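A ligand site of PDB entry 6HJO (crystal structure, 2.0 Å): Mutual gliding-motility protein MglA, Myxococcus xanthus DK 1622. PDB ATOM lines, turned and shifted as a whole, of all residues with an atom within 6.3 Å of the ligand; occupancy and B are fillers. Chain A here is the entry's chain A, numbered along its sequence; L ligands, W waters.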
ATOM      1  N   GLY A  19      14.691 -15.220   8.313  1.00  0.00           N
ATOM      2  CA  GLY A  19      13.350 -14.974   7.767  1.00  0.00           C
ATOM      3  C   GLY A  19      13.151 -15.731   6.481  1.00  0.00           C
ATOM      4  O   GLY A  19      14.118 -16.296   5.941  1.00  0.00           O
ATOM      5  N   PRO A  20      11.919 -15.752   5.926  1.00  0.00           N
ATOM      6  CA  PRO A  20      11.697 -16.494   4.666  1.00  0.00           C
ATOM      7  C   PRO A  20      12.517 -15.944   3.496  1.00  0.00           C
ATOM      8  O   PRO A  20      13.021 -14.826   3.541  1.00  0.00           O
ATOM      9  CB  PRO A  20      10.178 -16.345   4.428  1.00  0.00           C
ATOM     10  CG  PRO A  20       9.737 -15.224   5.270  1.00  0.00           C
ATOM     11  CD  PRO A  20      10.677 -15.133   6.437  1.00  0.00           C
ATOM     12  N   GLY A  21      12.625 -16.724   2.431  1.00  0.00           N
ATOM     13  CA  GLY A  21      13.334 -16.287   1.236  1.00  0.00           C
ATOM     14  C   GLY A  21      12.690 -15.024   0.694  1.00  0.00           C
ATOM     15  O   GLY A  21      11.462 -14.879   0.775  1.00  0.00           O
ATOM     16  N   LEU A  22      13.516 -14.073   0.214  1.00  0.00           N
ATOM     17  CA  LEU A  22      13.100 -12.804  -0.391  1.00  0.00           C
ATOM     18  C   LEU A  22      12.351 -11.826   0.556  1.00  0.00           C
ATOM     19  O   LEU A  22      11.669 -10.920   0.075  1.00  0.00           O
ATOM     20  CB  LEU A  22      12.290 -13.034  -1.705  1.00  0.00           C
ATOM     21  CG  LEU A  22      12.866 -14.067  -2.711  1.00  0.00           C
ATOM     22  CD1 LEU A  22      11.970 -14.165  -3.941  1.00  0.00           C
ATOM     23  CD2 LEU A  22      14.276 -13.720  -3.139  1.00  0.00           C
ATOM     24  N   CYS A  23      12.531 -11.947   1.874  1.00  0.00           N
ATOM     25  CA  CYS A  23      11.876 -11.068   2.852  1.00  0.00           C
ATOM     26  C   CYS A  23      12.582  -9.713   3.054  1.00  0.00           C
ATOM     27  O   CYS A  23      11.950  -8.791   3.587  1.00  0.00           O
ATOM     28  CB  CYS A  23      11.684 -11.795   4.177  1.00  0.00           C
ATOM     29  SG  CYS A  23      13.238 -12.119   5.056  1.00  0.00           S
ATOM     30  N   GLY A  24      13.863  -9.604   2.668  1.00  0.00           N
ATOM     31  CA  GLY A  24      14.629  -8.354   2.801  1.00  0.00           C
ATOM     32  C   GLY A  24      15.890  -8.422   3.649  1.00  0.00           C
ATOM     33  O   GLY A  24      16.400  -7.393   4.093  1.00  0.00           O
ATOM     34  N   LYS A  25      16.428  -9.635   3.861  1.00  0.00           N
ATOM     35  CA  LYS A  25      17.644  -9.823   4.667  1.00  0.00           C
ATOM     36  C   LYS A  25      18.902  -9.264   3.982  1.00  0.00           C
ATOM     37  O   LYS A  25      19.644  -8.516   4.608  1.00  0.00           O
ATOM     38  CB  LYS A  25      17.826 -11.305   5.046  1.00  0.00           C
ATOM     39  CG  LYS A  25      16.629 -11.914   5.775  1.00  0.00           C
ATOM     40  CD  LYS A  25      16.823 -13.399   6.147  1.00  0.00           C
ATOM     41  CE  LYS A  25      17.010 -14.328   4.964  1.00  0.00           C
ATOM     42  NZ  LYS A  25      15.824 -14.276   4.041  1.00  0.00           N
ATOM     43  N   THR A  26      19.088  -9.531   2.680  1.00  0.00           N
ATOM     44  CA  THR A  26      20.217  -8.973   1.906  1.00  0.00           C
ATOM     45  C   THR A  26      20.110  -7.452   1.912  1.00  0.00           C
ATOM     46  O   THR A  26      21.105  -6.766   2.122  1.00  0.00           O
ATOM     47  CB  THR A  26      20.179  -9.513   0.451  1.00  0.00           C
ATOM     48  OG1 THR A  26      20.334 -10.927   0.508  1.00  0.00           O
ATOM     49  CG2 THR A  26      21.238  -8.888  -0.451  1.00  0.00           C
ATOM     50  N   THR A  27      18.889  -6.929   1.710  1.00  0.00           N
ATOM     51  CA  THR A  27      18.622  -5.496   1.660  1.00  0.00           C
ATOM     52  C   THR A  27      19.063  -4.783   2.947  1.00  0.00           C
ATOM     53  O   THR A  27      19.718  -3.750   2.870  1.00  0.00           O
ATOM     54  CB  THR A  27      17.149  -5.225   1.269  1.00  0.00           C
ATOM     55  OG1 THR A  27      16.859  -5.933   0.076  1.00  0.00           O
ATOM     56  CG2 THR A  27      16.888  -3.781   1.006  1.00  0.00           C
ATOM     57  N   ASN A  28      18.711  -5.365   4.116  1.00  0.00           N
ATOM     58  CA  ASN A  28      19.085  -4.864   5.438  1.00  0.00           C
ATOM     59  C   ASN A  28      20.624  -4.813   5.549  1.00  0.00           C
ATOM     60  O   ASN A  28      21.177  -3.755   5.828  1.00  0.00           O
ATOM     61  CB  ASN A  28      18.528  -5.822   6.530  1.00  0.00           C
ATOM     62  CG  ASN A  28      17.199  -5.379   7.072  1.00  0.00           C
ATOM     63  OD1 ASN A  28      17.145  -4.552   7.996  1.00  0.00           O
ATOM     64  ND2 ASN A  28      16.114  -5.883   6.485  1.00  0.00           N
ATOM     65  N   GLN A  30      22.973  -4.952   3.132  1.00  0.00           N
ATOM     66  CA  GLN A  30      23.542  -4.044   2.115  1.00  0.00           C
ATOM     67  C   GLN A  30      23.353  -2.601   2.552  1.00  0.00           C
ATOM     68  O   GLN A  30      24.287  -1.815   2.433  1.00  0.00           O
ATOM     69  CB  GLN A  30      22.893  -4.241   0.744  1.00  0.00           C
ATOM     70  CG  GLN A  30      23.293  -5.512  -0.005  1.00  0.00           C
ATOM     71  CD  GLN A  30      22.573  -5.630  -1.339  1.00  0.00           C
ATOM     72  OE1 GLN A  30      21.499  -5.029  -1.580  1.00  0.00           O
ATOM     73  NE2 GLN A  30      23.116  -6.433  -2.239  1.00  0.00           N
ATOM     74  N   THR A  78      23.614 -13.855   7.111  1.00  0.00           N
ATOM     75  CA  THR A  78      22.293 -14.238   6.596  1.00  0.00           C
ATOM     76  C   THR A  78      22.423 -15.292   5.513  1.00  0.00           C
ATOM     77  O   THR A  78      23.468 -15.363   4.860  1.00  0.00           O
ATOM     78  CB  THR A  78      21.441 -13.008   6.141  1.00  0.00           C
ATOM     79  OG1 THR A  78      20.063 -13.350   6.187  1.00  0.00           O
ATOM     80  CG2 THR A  78      21.819 -12.471   4.742  1.00  0.00           C
ATOM     81  N   VAL A  79      21.379 -16.124   5.343  1.00  0.00           N
ATOM     82  CA  VAL A  79      21.273 -17.084   4.250  1.00  0.00           C
ATOM     83  C   VAL A  79      20.313 -16.392   3.256  1.00  0.00           C
ATOM     84  O   VAL A  79      19.121 -16.371   3.499  1.00  0.00           O
ATOM     85  CB  VAL A  79      20.763 -18.500   4.683  1.00  0.00           C
ATOM     86  CG1 VAL A  79      20.441 -19.352   3.452  1.00  0.00           C
ATOM     87  CG2 VAL A  79      21.772 -19.208   5.574  1.00  0.00           C
ATOM     88  N   PRO A  80      20.825 -15.715   2.205  1.00  0.00           N
ATOM     89  CA  PRO A  80      19.921 -14.992   1.286  1.00  0.00           C
ATOM     90  C   PRO A  80      19.210 -15.868   0.256  1.00  0.00           C
ATOM     91  O   PRO A  80      19.680 -16.968  -0.057  1.00  0.00           O
ATOM     92  CB  PRO A  80      20.885 -14.022   0.580  1.00  0.00           C
ATOM     93  CG  PRO A  80      22.183 -14.758   0.541  1.00  0.00           C
ATOM     94  CD  PRO A  80      22.247 -15.560   1.809  1.00  0.00           C
ATOM     95  N   GLY A  81      18.115 -15.333  -0.317  1.00  0.00           N
ATOM     96  CA  GLY A  81      17.367 -15.958  -1.394  1.00  0.00           C
ATOM     97  C   GLY A  81      16.587 -17.205  -1.018  1.00  0.00           C
ATOM     98  O   GLY A  81      16.355 -17.467   0.158  1.00  0.00           O
ATOM     99  N   GLN A  82      16.180 -17.975  -2.043  1.00  0.00           N
ATOM    100  CA  GLN A  82      15.461 -19.236  -1.868  1.00  0.00           C
ATOM    101  C   GLN A  82      16.398 -20.254  -1.189  1.00  0.00           C
ATOM    102  O   GLN A  82      17.587 -20.320  -1.524  1.00  0.00           O
ATOM    103  CB  GLN A  82      14.966 -19.776  -3.218  1.00  0.00           C
ATOM    104  CG  GLN A  82      13.847 -20.825  -3.078  1.00  0.00           C
ATOM    105  CD  GLN A  82      13.331 -21.403  -4.381  1.00  0.00           C
ATOM    106  OE1 GLN A  82      13.713 -21.009  -5.493  1.00  0.00           O
ATOM    107  NE2 GLN A  82      12.421 -22.361  -4.257  1.00  0.00           N
ATOM    108  N   VAL A 102      13.325 -11.118  10.167  1.00  0.00           N
ATOM    109  CA  VAL A 102      12.793 -10.198   9.156  1.00  0.00           C
ATOM    110  C   VAL A 102      11.540 -10.844   8.573  1.00  0.00           C
ATOM    111  O   VAL A 102      11.615 -11.889   7.908  1.00  0.00           O
ATOM    112  CB  VAL A 102      13.831  -9.834   8.064  1.00  0.00           C
ATOM    113  CG1 VAL A 102      13.222  -8.851   7.047  1.00  0.00           C
ATOM    114  CG2 VAL A 102      15.109  -9.237   8.663  1.00  0.00           C
ATOM    115  N   ASP A 104       8.245 -10.630   6.086  1.00  0.00           N
ATOM    116  CA  ASP A 104       7.765 -10.040   4.849  1.00  0.00           C
ATOM    117  C   ASP A 104       6.281  -9.683   5.111  1.00  0.00           C
ATOM    118  O   ASP A 104       5.470 -10.572   5.360  1.00  0.00           O
ATOM    119  CB  ASP A 104       7.919 -11.034   3.690  1.00  0.00           C
ATOM    120  CG  ASP A 104       7.588 -10.465   2.321  1.00  0.00           C
ATOM    121  OD1 ASP A 104       6.570  -9.721   2.206  1.00  0.00           O
ATOM    122  OD2 ASP A 104       8.335 -10.779   1.356  1.00  0.00           O
ATOM    123  N   ASN A 141       9.062  -5.963   7.703  1.00  0.00           N
ATOM    124  CA  ASN A 141       9.600  -5.346   6.503  1.00  0.00           C
ATOM    125  C   ASN A 141       8.557  -5.217   5.407  1.00  0.00           C
ATOM    126  O   ASN A 141       7.520  -5.879   5.474  1.00  0.00           O
ATOM    127  CB  ASN A 141      10.861  -6.106   6.016  1.00  0.00           C
ATOM    128  CG  ASN A 141      11.663  -5.343   5.007  1.00  0.00           C
ATOM    129  OD1 ASN A 141      11.777  -4.104   5.101  1.00  0.00           O
ATOM    130  ND2 ASN A 141      12.198  -6.032   3.994  1.00  0.00           N
ATOM    131  N   LYS A 142       8.848  -4.409   4.369  1.00  0.00           N
ATOM    132  CA  LYS A 142       7.958  -4.162   3.215  1.00  0.00           C
ATOM    133  C   LYS A 142       6.697  -3.427   3.620  1.00  0.00           C
ATOM    134  O   LYS A 142       5.631  -3.645   3.018  1.00  0.00           O
ATOM    135  CB  LYS A 142       7.635  -5.445   2.411  1.00  0.00           C
ATOM    136  CG  LYS A 142       8.819  -6.344   2.152  1.00  0.00           C
ATOM    137  CD  LYS A 142       8.671  -7.146   0.866  1.00  0.00           C
ATOM    138  CE  LYS A 142       9.932  -7.958   0.706  1.00  0.00           C
ATOM    139  NZ  LYS A 142       9.761  -9.019  -0.319  1.00  0.00           N
ATOM    140  N   ARG A 143       6.830  -2.467   4.586  1.00  0.00           N
ATOM    141  CA  ARG A 143       5.685  -1.631   5.027  1.00  0.00           C
ATOM    142  C   ARG A 143       5.135  -0.699   3.920  1.00  0.00           C
ATOM    143  O   ARG A 143       4.003  -0.229   4.024  1.00  0.00           O
ATOM    144  CB  ARG A 143       6.017  -0.825   6.301  1.00  0.00           C
ATOM    145  CG  ARG A 143       6.402  -1.670   7.547  1.00  0.00           C
ATOM    146  CD  ARG A 143       5.391  -2.743   7.945  1.00  0.00           C
ATOM    147  NE  ARG A 143       4.003  -2.253   7.983  1.00  0.00           N
ATOM    148  CZ  ARG A 143       2.934  -3.019   7.869  1.00  0.00           C
ATOM    149  NH1 ARG A 143       3.053  -4.337   7.724  1.00  0.00           N
ATOM    150  NH2 ARG A 143       1.712  -2.490   7.923  1.00  0.00           N
ATOM    151  N   ASP A 144       5.928  -0.469   2.855  1.00  0.00           N
ATOM    152  CA  ASP A 144       5.554   0.387   1.714  1.00  0.00           C
ATOM    153  C   ASP A 144       4.498  -0.226   0.754  1.00  0.00           C
ATOM    154  O   ASP A 144       3.815   0.508   0.057  1.00  0.00           O
ATOM    155  CB  ASP A 144       6.829   0.721   0.909  1.00  0.00           C
ATOM    156  CG  ASP A 144       7.532  -0.508   0.339  1.00  0.00           C
ATOM    157  OD1 ASP A 144       7.904  -1.404   1.141  1.00  0.00           O
ATOM    158  OD2 ASP A 144       7.669  -0.590  -0.891  1.00  0.00           O
ATOM    159  N   LEU A 145       4.421  -1.570   0.699  1.00  0.00           N
ATOM    160  CA  LEU A 145       3.591  -2.293  -0.273  1.00  0.00           C
ATOM    161  C   LEU A 145       2.090  -2.232  -0.017  1.00  0.00           C
ATOM    162  O   LEU A 145       1.662  -2.223   1.139  1.00  0.00           O
ATOM    163  CB  LEU A 145       4.058  -3.754  -0.446  1.00  0.00           C
ATOM    164  CG  LEU A 145       5.438  -3.945  -1.088  1.00  0.00           C
ATOM    165  CD1 LEU A 145       5.879  -5.374  -1.000  1.00  0.00           C
ATOM    166  CD2 LEU A 145       5.473  -3.477  -2.562  1.00  0.00           C
ATOM    167  N   ALA A 168       9.776  -1.494   8.947  1.00  0.00           N
ATOM    168  CA  ALA A 168      10.825  -1.123   8.011  1.00  0.00           C
ATOM    169  C   ALA A 168      10.412  -1.139   6.560  1.00  0.00           C
ATOM    170  O   ALA A 168       9.459  -1.805   6.185  1.00  0.00           O
ATOM    171  CB  ALA A 168      12.033  -2.036   8.208  1.00  0.00           C
ATOM    172  N   VAL A 169      11.183  -0.421   5.739  1.00  0.00           N
ATOM    173  CA  VAL A 169      11.177  -0.399   4.274  1.00  0.00           C
ATOM    174  C   VAL A 169      12.690  -0.462   4.010  1.00  0.00           C
ATOM    175  O   VAL A 169      13.361   0.568   3.906  1.00  0.00           O
ATOM    176  CB  VAL A 169      10.514   0.834   3.636  1.00  0.00           C
ATOM    177  CG1 VAL A 169      10.644   0.793   2.098  1.00  0.00           C
ATOM    178  CG2 VAL A 169       9.033   0.932   4.040  1.00  0.00           C
ATOM    179  N   ALA A 170      13.228  -1.674   4.028  1.00  0.00           N
ATOM    180  CA  ALA A 170      14.676  -1.918   3.932  1.00  0.00           C
ATOM    181  C   ALA A 170      15.400  -1.205   2.733  1.00  0.00           C
ATOM    182  O   ALA A 170      16.452  -0.629   2.975  1.00  0.00           O
ATOM    183  CB  ALA A 170      14.969  -3.416   3.927  1.00  0.00           C
ATOM    184  N   PRO A 171      14.836  -1.152   1.485  1.00  0.00           N
ATOM    185  CA  PRO A 171      15.560  -0.486   0.367  1.00  0.00           C
ATOM    186  C   PRO A 171      15.833   0.994   0.578  1.00  0.00           C
ATOM    187  O   PRO A 171      16.808   1.484   0.035  1.00  0.00           O
ATOM    188  CB  PRO A 171      14.661  -0.740  -0.854  1.00  0.00           C
ATOM    189  CG  PRO A 171      13.830  -1.889  -0.509  1.00  0.00           C
ATOM    190  CD  PRO A 171      13.588  -1.763   0.974  1.00  0.00           C
HETATM  191  P1  LIG L   1      16.479 -12.038   1.157  1.00  0.00           P
HETATM  192  O1  LIG L   1      16.296 -13.297   0.373  1.00  0.00           O
HETATM  193  O2  LIG L   1      15.769 -12.034   2.435  1.00  0.00           O
HETATM  194  O3  LIG L   1      17.920 -11.682   1.278  1.00  0.00           O
HETATM  195  O4  LIG L   1      15.767 -10.882   0.302  1.00  0.00           O
HETATM  196  P2  LIG L   1      16.219  -9.583  -0.503  1.00  0.00           P
HETATM  197  O5  LIG L   1      17.120  -9.939  -1.598  1.00  0.00           O
HETATM  198  O6  LIG L   1      16.807  -8.556   0.460  1.00  0.00           O
HETATM  199  O7  LIG L   1      14.790  -9.044  -1.046  1.00  0.00           O
HETATM  200  C1  LIG L   1      14.096  -9.682  -2.143  1.00  0.00           C
HETATM  201  C2  LIG L   1      13.380  -8.621  -2.958  1.00  0.00           C
HETATM  202  O8  LIG L   1      12.498  -7.860  -2.112  1.00  0.00           O
HETATM  203  C3  LIG L   1      14.274  -7.610  -3.678  1.00  0.00           C
HETATM  204  O9  LIG L   1      13.708  -7.317  -4.946  1.00  0.00           O
HETATM  205  C4  LIG L   1      14.226  -6.404  -2.730  1.00  0.00           C
HETATM  206  O10 LIG L   1      14.487  -5.139  -3.332  1.00  0.00           O
HETATM  207  C5  LIG L   1      12.784  -6.486  -2.247  1.00  0.00           C
HETATM  208  N1  LIG L   1      12.544  -5.820  -0.964  1.00  0.00           N
HETATM  209  C6  LIG L   1      13.244  -5.977   0.210  1.00  0.00           C
HETATM  210  N2  LIG L   1      12.772  -5.239   1.186  1.00  0.00           N
HETATM  211  C7  LIG L   1      11.709  -4.548   0.621  1.00  0.00           C
HETATM  212  C8  LIG L   1      10.809  -3.587   1.168  1.00  0.00           C
HETATM  213  O11 LIG L   1      10.834  -3.116   2.301  1.00  0.00           O
HETATM  214  N3  LIG L   1       9.867  -3.154   0.248  1.00  0.00           N
HETATM  215  C9  LIG L   1       9.802  -3.562  -1.057  1.00  0.00           C
HETATM  216  N4  LIG L   1       8.825  -3.047  -1.810  1.00  0.00           N
HETATM  217  N5  LIG L   1      10.658  -4.439  -1.592  1.00  0.00           N
HETATM  218  C10 LIG L   1      11.571  -4.893  -0.710  1.00  0.00           C
HETATM  219  O   HOH W   1      18.588  -8.310  -3.194  1.00  0.00           O
HETATM  220  O   HOH W   2      12.733  -2.676  -4.252  1.00  0.00           O
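The side-chain sulfur of Cys 23 sits close to the side-chain amino group of Lys 25 (3.5 Å).
O of Gly 19 sits at hydrogen-bond distance from NZ of Lys 25.
The backbone carbonyl oxygen of Leu 22 sits at hydrogen-bond distance from the side-chain amino group of Lys 142 (2.7 Å).
The side-chain amide oxygen (OD1) of Asn 141 lies within hydrogen-bond range of the backbone NH (N) of Ala 170 (3.0 Å).
The backbone carbonyl oxygen (O) of Cys 23 sits at hydrogen-bond distance from the side-chain amide nitrogen (ND2) of Asn 141, 2.8 Å away.
The side-chain amide oxygen (OD1) of Asn 141 sits close to the backbone carbonyl oxygen (O) of Ala 168, 3.4 Å away.
The backbone NH (N) of Lys 142 sits at hydrogen-bond distance from the backbone carbonyl oxygen (O) of Ala 168 (3.2 Å).
The backbone carbonyl oxygen of Val 102 sits at hydrogen-bond distance from the side-chain sulfur of Cys 23, 3.3 Å away.
Pro 80 touches the ligand.
CD2 of Leu 145 touches N4 of the ligand, at 3.5 Å.
CA of Val 169 touches O11 of the ligand, 3.4 Å away.
Pro 171 touches the ligand (CD to C8, 3.3 Å).
Hydrophobic or aromatic side chains within 4 Å of the ligand: Leu 22, Pro 80, Leu 145, Val 169, Ala 170 and Pro 171.
Of the 27 residues printed, 15 come within 4 Å of the ligand.
The nearest printed residue that does not touch the ligand is Gly 21 (4.01 Å).
The backbone NH (N) of Thr 26 is in hydrogen-bond range of an oxygen (O3) of the ligand, 2.8 Å away.
An oxygen (O3) of the ligand sits at hydrogen-bond distance from the side-chain hydroxyl (OG1) of Thr 26 (2.6 Å).
N of Thr 27 sits at hydrogen-bond distance from O6 of the ligand (2.9 Å).
OG1 of Thr 27 is in hydrogen-bond range of O6 of the ligand (2.7 Å).
The backbone NH (N) of Lys 25 sits at hydrogen-bond distance from an oxygen (O2) of the ligand (2.9 Å).
The side-chain amino group of Lys 25 is in salt-bridge range of an oxygen (O2) of the ligand.
OD1 of Asp 144 is in hydrogen-bond range of N3 of the ligand (2.8 Å).
The backbone NH of Gly 81 is in hydrogen-bond range of an oxygen (O1) of the ligand.
An oxygen (O1) of the ligand is in hydrogen-bond range of the backbone NH (N) of Leu 22 (2.9 Å).
ND2 of Asn 141 lies within hydrogen-bond range of N2 of the ligand, at 3.0 Å.
The backbone NH of Gly 24 sits at hydrogen-bond distance from an oxygen (O2) of the ligand (3.1 Å).
The backbone NH of Lys 142 lies within hydrogen-bond range of an oxygen (O11) of the ligand, 3.1 Å away.
NZ of Lys 142 sits at hydrogen-bond distance from O8 of the ligand (3.5 Å).
The backbone NH of Ala 170 lies within hydrogen-bond range of an oxygen (O11) of the ligand (3.3 Å).
The backbone NH (N) of Cys 23 sits at hydrogen-bond distance from an oxygen (O2) of the ligand (3.3 Å).
The side-chain sulfur of Cys 23 is in hydrogen-bond range of an oxygen (O2) of the ligand (3.6 Å).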
